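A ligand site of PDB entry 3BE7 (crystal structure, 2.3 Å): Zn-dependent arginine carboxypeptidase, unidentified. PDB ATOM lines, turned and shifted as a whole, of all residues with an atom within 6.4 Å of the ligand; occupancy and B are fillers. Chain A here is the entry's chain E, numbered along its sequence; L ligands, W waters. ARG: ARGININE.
N of Met 192 is in hydrogen-bond range of OXT of the ligand, at 2.8 Å. The side-chain carboxylate (OE1) of Glu 291 is in salt-bridge range of a nitrogen (NE) of the ligand (2.7 Å). NE2 of His 227 lies within hydrogen-bond range of O of the ligand, 2.8 Å away. The backbone NH (N) of Val 191 lies within hydrogen-bond range of an oxygen (O) of the ligand, at 2.6 Å. The side-chain carboxylate of Asp 267 is in salt-bridge range of a nitrogen (NH1) of the ligand, at 3.4 Å. The side-chain carboxylate of Asp 317 is in salt-bridge range of a nitrogen (N) of the ligand (2.8 Å). The side-chain amide oxygen of Gln 298 sits at hydrogen-bond distance from a nitrogen (NH1) of the ligand, 2.8 Å away. The backbone carbonyl oxygen (O) of Asp 267 is in hydrogen-bond range of a nitrogen (NH1) of the ligand, 3.2 Å away.
The side-chain hydroxyl (OG) of Ser 247 sits at hydrogen-bond distance from a ring nitrogen (ND1) of His 227. N of Asp 317 is in hydrogen-bond range of O of His 64. The side-chain carboxylate (OD1) of Asp 267 sits at hydrogen-bond distance from the side-chain amide nitrogen (NE2) of Gln 298, at 3.0 Å. A ring nitrogen (ND1) of His 144 is in hydrogen-bond range of the side-chain hydroxyl (OG) of Ser 193 (2.8 Å). ND1 of His 245 sits at hydrogen-bond distance from OD1 of Asp 267 (2.8 Å). The side-chain amide nitrogen (NE2) of Gln 298 sits at hydrogen-bond distance from the backbone carbonyl oxygen (O) of His 245 (2.9 Å). A ring nitrogen (ND1) of His 225 sits at hydrogen-bond distance from a ring nitrogen (NE2) of His 245. The side-chain hydroxyl (OG) of Ser 271 is in hydrogen-bond range of the side-chain carboxylate (OE2) of Glu 291 (2.9 Å).
Water W1 lies within hydrogen-bond range of NE2 of His 64 (2.8 Å), NE2 of His 66 (2.8 Å), OD2 of Asp 317 (2.8 Å) and N of the ligand (3.0 Å).
His 144 touches the ligand (CE1 to OXT, 3.2 Å). CA of Gly 190 touches O of the ligand, at 3.2 Å. His 225 touches the ligand (CE1 to O, 3.4 Å). His 245 touches the ligand (NE2 to CA, 3.5 Å). Val 270 touches the ligand (CG1 to CD, 3.7 Å). Ile 274 touches the ligand. CG1 of Val 294 touches NH2 of the ligand (3.5 Å). Gly 295 touches the ligand. Ile 320 touches the ligand. Hydrophobic or aromatic side chains within 4 Å of the ligand: His 144, Val 191, Met 192, His 225, His 227, His 245, Val 270, Ile 274, Val 294 and Ile 320. 16 residues have an atom within 4 Å of the ligand: His 144, Gly 190, Val 191, Met 192, His 225, His 227, His 245, Asp 267, Val 270, Ile 274, Glu 291, Val 294, Gly 295, Gln 298, Asp 317 and Ile 320. The nearest printed residue that does not touch the ligand is Ser 271 (4.1 Å).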
ATOM      1  N   HIS A  64     -21.258 -21.471 -10.900  1.00  0.00           N
ATOM      2  CA  HIS A  64     -21.581 -20.043 -11.047  1.00  0.00           C
ATOM      3  C   HIS A  64     -20.984 -19.511 -12.345  1.00  0.00           C
ATOM      4  O   HIS A  64     -19.857 -19.027 -12.361  1.00  0.00           O
ATOM      5  CB  HIS A  64     -21.051 -19.248  -9.847  1.00  0.00           C
ATOM      6  CG  HIS A  64     -21.619 -17.863  -9.729  1.00  0.00           C
ATOM      7  ND1 HIS A  64     -22.417 -17.465  -8.680  1.00  0.00           N
ATOM      8  CD2 HIS A  64     -21.478 -16.776 -10.526  1.00  0.00           C
ATOM      9  CE1 HIS A  64     -22.757 -16.205  -8.840  1.00  0.00           C
ATOM     10  NE2 HIS A  64     -22.205 -15.752  -9.944  1.00  0.00           N
ATOM     11  N   HIS A  66     -22.032 -17.241 -16.180  1.00  0.00           N
ATOM     12  CA  HIS A  66     -22.973 -16.520 -17.029  1.00  0.00           C
ATOM     13  C   HIS A  66     -22.576 -16.655 -18.483  1.00  0.00           C
ATOM     14  O   HIS A  66     -21.847 -15.817 -19.024  1.00  0.00           O
ATOM     15  CB  HIS A  66     -23.037 -15.040 -16.641  1.00  0.00           C
ATOM     16  CG  HIS A  66     -23.580 -14.789 -15.264  1.00  0.00           C
ATOM     17  ND1 HIS A  66     -24.929 -14.648 -15.012  1.00  0.00           N
ATOM     18  CD2 HIS A  66     -22.953 -14.645 -14.077  1.00  0.00           C
ATOM     19  CE1 HIS A  66     -25.115 -14.434 -13.726  1.00  0.00           C
ATOM     20  NE2 HIS A  66     -23.925 -14.420 -13.131  1.00  0.00           N
ATOM     21  N   HIS A 144     -29.042  -5.690  -6.729  1.00  0.00           N
ATOM     22  CA  HIS A 144     -27.875  -6.101  -7.505  1.00  0.00           C
ATOM     23  C   HIS A 144     -28.263  -6.552  -8.899  1.00  0.00           C
ATOM     24  O   HIS A 144     -27.611  -6.203  -9.876  1.00  0.00           O
ATOM     25  CB  HIS A 144     -27.099  -7.207  -6.778  1.00  0.00           C
ATOM     26  CG  HIS A 144     -25.981  -7.776  -7.583  1.00  0.00           C
ATOM     27  ND1 HIS A 144     -24.892  -7.025  -7.975  1.00  0.00           N
ATOM     28  CD2 HIS A 144     -25.779  -9.014  -8.091  1.00  0.00           C
ATOM     29  CE1 HIS A 144     -24.068  -7.780  -8.681  1.00  0.00           C
ATOM     30  NE2 HIS A 144     -24.586  -8.998  -8.762  1.00  0.00           N
ATOM     31  N   GLY A 189     -26.231  -6.416  -1.912  1.00  0.00           N
ATOM     32  CA  GLY A 189     -25.587  -5.753  -3.038  1.00  0.00           C
ATOM     33  C   GLY A 189     -24.379  -6.490  -3.573  1.00  0.00           C
ATOM     34  O   GLY A 189     -23.929  -7.504  -3.019  1.00  0.00           O
ATOM     35  N   GLY A 190     -23.837  -5.976  -4.673  1.00  0.00           N
ATOM     36  CA  GLY A 190     -22.786  -6.672  -5.394  1.00  0.00           C
ATOM     37  C   GLY A 190     -21.673  -5.768  -5.860  1.00  0.00           C
ATOM     38  O   GLY A 190     -21.736  -4.539  -5.683  1.00  0.00           O
ATOM     39  N   VAL A 191     -20.657  -6.375  -6.470  1.00  0.00           N
ATOM     40  CA  VAL A 191     -19.476  -5.661  -6.900  1.00  0.00           C
ATOM     41  C   VAL A 191     -19.737  -4.954  -8.225  1.00  0.00           C
ATOM     42  O   VAL A 191     -19.486  -3.760  -8.354  1.00  0.00           O
ATOM     43  CB  VAL A 191     -18.242  -6.619  -6.978  1.00  0.00           C
ATOM     44  CG1 VAL A 191     -17.029  -5.908  -7.562  1.00  0.00           C
ATOM     45  CG2 VAL A 191     -17.896  -7.154  -5.601  1.00  0.00           C
ATOM     46  N   MET A 192     -20.285  -5.689  -9.184  1.00  0.00           N
ATOM     47  CA  MET A 192     -20.274  -5.279 -10.595  1.00  0.00           C
ATOM     48  C   MET A 192     -21.431  -4.359 -10.984  1.00  0.00           C
ATOM     49  O   MET A 192     -21.493  -3.881 -12.119  1.00  0.00           O
ATOM     50  CB  MET A 192     -20.225  -6.509 -11.515  1.00  0.00           C
ATOM     51  CG  MET A 192     -18.952  -7.361 -11.411  1.00  0.00           C
ATOM     52  SD  MET A 192     -17.407  -6.473 -11.730  1.00  0.00           S
ATOM     53  CE  MET A 192     -17.615  -6.032 -13.453  1.00  0.00           C
ATOM     54  N   SER A 193     -22.328  -4.105 -10.045  1.00  0.00           N
ATOM     55  CA  SER A 193     -23.519  -3.290 -10.291  1.00  0.00           C
ATOM     56  C   SER A 193     -23.332  -1.865  -9.774  1.00  0.00           C
ATOM     57  O   SER A 193     -22.584  -1.631  -8.833  1.00  0.00           O
ATOM     58  CB  SER A 193     -24.740  -3.931  -9.644  1.00  0.00           C
ATOM     59  OG  SER A 193     -24.457  -4.328  -8.307  1.00  0.00           O
ATOM     60  N   VAL A 198     -22.693  -3.541  -0.830  1.00  0.00           N
ATOM     61  CA  VAL A 198     -22.216  -4.900  -0.579  1.00  0.00           C
ATOM     62  C   VAL A 198     -22.577  -5.439   0.821  1.00  0.00           C
ATOM     63  O   VAL A 198     -22.830  -6.635   1.000  1.00  0.00           O
ATOM     64  CB  VAL A 198     -20.697  -4.981  -0.905  1.00  0.00           C
ATOM     65  CG1 VAL A 198     -19.916  -5.835   0.078  1.00  0.00           C
ATOM     66  CG2 VAL A 198     -20.480  -5.436  -2.340  1.00  0.00           C
ATOM     67  N   HIS A 225     -27.046 -15.054  -4.282  1.00  0.00           N
ATOM     68  CA  HIS A 225     -25.983 -14.058  -4.250  1.00  0.00           C
ATOM     69  C   HIS A 225     -25.979 -13.361  -2.892  1.00  0.00           C
ATOM     70  O   HIS A 225     -26.975 -12.771  -2.511  1.00  0.00           O
ATOM     71  CB  HIS A 225     -26.193 -13.047  -5.385  1.00  0.00           C
ATOM     72  CG  HIS A 225     -25.325 -11.818  -5.304  1.00  0.00           C
ATOM     73  ND1 HIS A 225     -24.217 -11.660  -6.096  1.00  0.00           N
ATOM     74  CD2 HIS A 225     -25.432 -10.702  -4.563  1.00  0.00           C
ATOM     75  CE1 HIS A 225     -23.654 -10.496  -5.826  1.00  0.00           C
ATOM     76  NE2 HIS A 225     -24.373  -9.889  -4.888  1.00  0.00           N
ATOM     77  N   HIS A 227     -22.887 -11.230  -0.430  1.00  0.00           N
ATOM     78  CA  HIS A 227     -21.590 -10.794   0.073  1.00  0.00           C
ATOM     79  C   HIS A 227     -21.627 -10.451   1.562  1.00  0.00           C
ATOM     80  O   HIS A 227     -20.900 -11.050   2.353  1.00  0.00           O
ATOM     81  CB  HIS A 227     -21.087  -9.573  -0.711  1.00  0.00           C
ATOM     82  CG  HIS A 227     -20.588  -9.907  -2.089  1.00  0.00           C
ATOM     83  ND1 HIS A 227     -19.370 -10.511  -2.321  1.00  0.00           N
ATOM     84  CD2 HIS A 227     -21.139  -9.697  -3.308  1.00  0.00           C
ATOM     85  CE1 HIS A 227     -19.204 -10.668  -3.620  1.00  0.00           C
ATOM     86  NE2 HIS A 227     -20.259 -10.184  -4.244  1.00  0.00           N
ATOM     87  N   HIS A 245     -20.786 -16.399  -3.607  1.00  0.00           N
ATOM     88  CA  HIS A 245     -19.732 -15.533  -3.043  1.00  0.00           C
ATOM     89  C   HIS A 245     -19.420 -15.719  -1.565  1.00  0.00           C
ATOM     90  O   HIS A 245     -18.283 -16.052  -1.222  1.00  0.00           O
ATOM     91  CB  HIS A 245     -19.904 -14.059  -3.421  1.00  0.00           C
ATOM     92  CG  HIS A 245     -20.485 -13.855  -4.789  1.00  0.00           C
ATOM     93  ND1 HIS A 245     -19.827 -14.241  -5.931  1.00  0.00           N
ATOM     94  CD2 HIS A 245     -21.676 -13.358  -5.182  1.00  0.00           C
ATOM     95  CE1 HIS A 245     -20.583 -13.968  -6.982  1.00  0.00           C
ATOM     96  NE2 HIS A 245     -21.707 -13.430  -6.554  1.00  0.00           N
ATOM     97  N   SER A 247     -18.940 -13.786   1.013  1.00  0.00           N
ATOM     98  CA  SER A 247     -17.643 -13.144   1.191  1.00  0.00           C
ATOM     99  C   SER A 247     -17.318 -12.730   2.622  1.00  0.00           C
ATOM    100  O   SER A 247     -16.150 -12.707   2.999  1.00  0.00           O
ATOM    101  CB  SER A 247     -17.532 -11.935   0.264  1.00  0.00           C
ATOM    102  OG  SER A 247     -17.603 -12.347  -1.091  1.00  0.00           O
ATOM    103  N   ASP A 267     -16.098 -17.689  -5.201  1.00  0.00           N
ATOM    104  CA  ASP A 267     -15.407 -17.433  -6.461  1.00  0.00           C
ATOM    105  C   ASP A 267     -14.164 -16.576  -6.249  1.00  0.00           C
ATOM    106  O   ASP A 267     -14.200 -15.348  -6.356  1.00  0.00           O
ATOM    107  CB  ASP A 267     -16.360 -16.808  -7.487  1.00  0.00           C
ATOM    108  CG  ASP A 267     -17.086 -15.575  -6.977  1.00  0.00           C
ATOM    109  OD1 ASP A 267     -17.372 -15.485  -5.755  1.00  0.00           O
ATOM    110  OD2 ASP A 267     -17.375 -14.682  -7.791  1.00  0.00           O
ATOM    111  N   ILE A 268     -13.058 -17.244  -5.944  1.00  0.00           N
ATOM    112  CA  ILE A 268     -11.922 -16.586  -5.301  1.00  0.00           C
ATOM    113  C   ILE A 268     -10.742 -16.307  -6.228  1.00  0.00           C
ATOM    114  O   ILE A 268      -9.696 -15.829  -5.790  1.00  0.00           O
ATOM    115  CB  ILE A 268     -11.489 -17.320  -4.009  1.00  0.00           C
ATOM    116  CG1 ILE A 268     -11.162 -18.796  -4.290  1.00  0.00           C
ATOM    117  CG2 ILE A 268     -12.560 -17.172  -2.921  1.00  0.00           C
ATOM    118  CD1 ILE A 268     -10.233 -19.429  -3.283  1.00  0.00           C
ATOM    119  N   VAL A 270     -11.481 -14.511  -9.320  1.00  0.00           N
ATOM    120  CA  VAL A 270     -11.916 -13.415 -10.194  1.00  0.00           C
ATOM    121  C   VAL A 270     -11.534 -12.008  -9.691  1.00  0.00           C
ATOM    122  O   VAL A 270     -11.428 -11.065 -10.494  1.00  0.00           O
ATOM    123  CB  VAL A 270     -13.443 -13.539 -10.545  1.00  0.00           C
ATOM    124  CG1 VAL A 270     -14.304 -13.388  -9.315  1.00  0.00           C
ATOM    125  CG2 VAL A 270     -13.868 -12.572 -11.639  1.00  0.00           C
ATOM    126  N   SER A 271     -11.276 -11.886  -8.393  1.00  0.00           N
ATOM    127  CA  SER A 271     -10.741 -10.648  -7.782  1.00  0.00           C
ATOM    128  C   SER A 271      -9.481 -10.141  -8.472  1.00  0.00           C
ATOM    129  O   SER A 271      -9.345  -8.947  -8.720  1.00  0.00           O
ATOM    130  CB  SER A 271     -10.474 -10.863  -6.292  1.00  0.00           C
ATOM    131  OG  SER A 271     -10.185  -9.650  -5.636  1.00  0.00           O
ATOM    132  N   ILE A 274     -10.476  -8.643 -11.829  1.00  0.00           N
ATOM    133  CA  ILE A 274     -11.159  -7.358 -11.710  1.00  0.00           C
ATOM    134  C   ILE A 274     -10.159  -6.247 -11.396  1.00  0.00           C
ATOM    135  O   ILE A 274     -10.156  -5.199 -12.047  1.00  0.00           O
ATOM    136  CB  ILE A 274     -12.298  -7.408 -10.666  1.00  0.00           C
ATOM    137  CG1 ILE A 274     -13.383  -8.387 -11.124  1.00  0.00           C
ATOM    138  CG2 ILE A 274     -12.924  -6.017 -10.463  1.00  0.00           C
ATOM    139  CD1 ILE A 274     -14.190  -9.008  -9.998  1.00  0.00           C
ATOM    140  N   GLU A 291     -14.723  -3.986  -5.052  1.00  0.00           N
ATOM    141  CA  GLU A 291     -13.943  -5.211  -5.150  1.00  0.00           C
ATOM    142  C   GLU A 291     -12.836  -5.280  -4.094  1.00  0.00           C
ATOM    143  O   GLU A 291     -12.581  -6.341  -3.511  1.00  0.00           O
ATOM    144  CB  GLU A 291     -13.351  -5.378  -6.554  1.00  0.00           C
ATOM    145  CG  GLU A 291     -12.662  -6.720  -6.821  1.00  0.00           C
ATOM    146  CD  GLU A 291     -13.453  -7.917  -6.304  1.00  0.00           C
ATOM    147  OE1 GLU A 291     -14.613  -8.096  -6.723  1.00  0.00           O
ATOM    148  OE2 GLU A 291     -12.897  -8.671  -5.477  1.00  0.00           O
ATOM    149  N   VAL A 294     -13.906  -6.654  -0.783  1.00  0.00           N
ATOM    150  CA  VAL A 294     -14.538  -7.963  -0.805  1.00  0.00           C
ATOM    151  C   VAL A 294     -13.499  -9.083  -0.937  1.00  0.00           C
ATOM    152  O   VAL A 294     -13.528 -10.049  -0.167  1.00  0.00           O
ATOM    153  CB  VAL A 294     -15.625  -8.045  -1.937  1.00  0.00           C
ATOM    154  CG1 VAL A 294     -16.049  -9.466  -2.204  1.00  0.00           C
ATOM    155  CG2 VAL A 294     -16.832  -7.226  -1.567  1.00  0.00           C
ATOM    156  N   GLY A 295     -12.577  -8.907  -1.880  1.00  0.00           N
ATOM    157  CA  GLY A 295     -11.793 -10.007  -2.447  1.00  0.00           C
ATOM    158  C   GLY A 295     -10.808 -10.670  -1.506  1.00  0.00           C
ATOM    159  O   GLY A 295     -10.721 -11.898  -1.455  1.00  0.00           O
ATOM    160  N   LYS A 296     -10.059  -9.847  -0.757  1.00  0.00           N
ATOM    161  CA  LYS A 296      -9.111 -10.333   0.253  1.00  0.00           C
ATOM    162  C   LYS A 296      -9.840 -11.074   1.379  1.00  0.00           C
ATOM    163  O   LYS A 296      -9.436 -12.165   1.775  1.00  0.00           O
ATOM    164  CB  LYS A 296      -8.300  -9.166   0.822  1.00  0.00           C
ATOM    165  CG  LYS A 296      -7.271  -9.546   1.878  1.00  0.00           C
ATOM    166  CD  LYS A 296      -6.432  -8.330   2.284  1.00  0.00           C
ATOM    167  CE  LYS A 296      -6.334  -8.204   3.794  1.00  0.00           C
ATOM    168  NZ  LYS A 296      -5.166  -8.942   4.354  1.00  0.00           N
ATOM    169  N   GLN A 298     -12.910 -12.355   1.358  1.00  0.00           N
ATOM    170  CA  GLN A 298     -13.531 -13.577   0.835  1.00  0.00           C
ATOM    171  C   GLN A 298     -12.562 -14.764   0.872  1.00  0.00           C
ATOM    172  O   GLN A 298     -12.953 -15.861   1.276  1.00  0.00           O
ATOM    173  CB  GLN A 298     -14.049 -13.367  -0.587  1.00  0.00           C
ATOM    174  CG  GLN A 298     -14.891 -14.537  -1.111  1.00  0.00           C
ATOM    175  CD  GLN A 298     -15.204 -14.459  -2.600  1.00  0.00           C
ATOM    176  OE1 GLN A 298     -14.530 -13.764  -3.366  1.00  0.00           O
ATOM    177  NE2 GLN A 298     -16.227 -15.188  -3.009  1.00  0.00           N
ATOM    178  N   ASP A 317     -17.767 -17.315 -11.216  1.00  0.00           N
ATOM    179  CA  ASP A 317     -18.275 -16.166 -11.982  1.00  0.00           C
ATOM    180  C   ASP A 317     -17.586 -15.961 -13.327  1.00  0.00           C
ATOM    181  O   ASP A 317     -17.149 -14.848 -13.643  1.00  0.00           O
ATOM    182  CB  ASP A 317     -18.327 -14.879 -11.158  1.00  0.00           C
ATOM    183  CG  ASP A 317     -19.576 -14.054 -11.441  1.00  0.00           C
ATOM    184  OD1 ASP A 317     -20.276 -14.321 -12.443  1.00  0.00           O
ATOM    185  OD2 ASP A 317     -19.862 -13.140 -10.648  1.00  0.00           O
ATOM    186  N   ILE A 320     -17.294 -12.725 -16.211  1.00  0.00           N
ATOM    187  CA  ILE A 320     -16.517 -11.543 -15.854  1.00  0.00           C
ATOM    188  C   ILE A 320     -15.158 -11.611 -16.528  1.00  0.00           C
ATOM    189  O   ILE A 320     -14.834 -10.773 -17.364  1.00  0.00           O
ATOM    190  CB  ILE A 320     -16.377 -11.380 -14.319  1.00  0.00           C
ATOM    191  CG1 ILE A 320     -17.762 -11.267 -13.673  1.00  0.00           C
ATOM    192  CG2 ILE A 320     -15.507 -10.159 -13.993  1.00  0.00           C
ATOM    193  CD1 ILE A 320     -17.766 -10.943 -12.202  1.00  0.00           C
HETATM  194  N   ARG L   1     -21.272 -11.052  -9.472  1.00  0.00           N
HETATM  195  CA  ARG L   1     -20.452 -10.668  -8.295  1.00  0.00           C
HETATM  196  C   ARG L   1     -20.761  -9.233  -7.907  1.00  0.00           C
HETATM  197  O   ARG L   1     -20.841  -8.908  -6.715  1.00  0.00           O
HETATM  198  CB  ARG L   1     -18.967 -10.807  -8.611  1.00  0.00           C
HETATM  199  CG  ARG L   1     -18.043 -10.576  -7.418  1.00  0.00           C
HETATM  200  CD  ARG L   1     -16.626 -10.934  -7.774  1.00  0.00           C
HETATM  201  NE  ARG L   1     -15.678 -10.526  -6.747  1.00  0.00           N
HETATM  202  CZ  ARG L   1     -15.221 -11.315  -5.773  1.00  0.00           C
HETATM  203  NH1 ARG L   1     -15.641 -12.575  -5.678  1.00  0.00           N
HETATM  204  NH2 ARG L   1     -14.358 -10.850  -4.898  1.00  0.00           N
HETATM  205  OXT ARG L   1     -20.914  -8.369  -8.767  1.00  0.00           O
HETATM  206  O   HOH W   1     -22.683 -13.234 -10.965  1.00  0.00           O
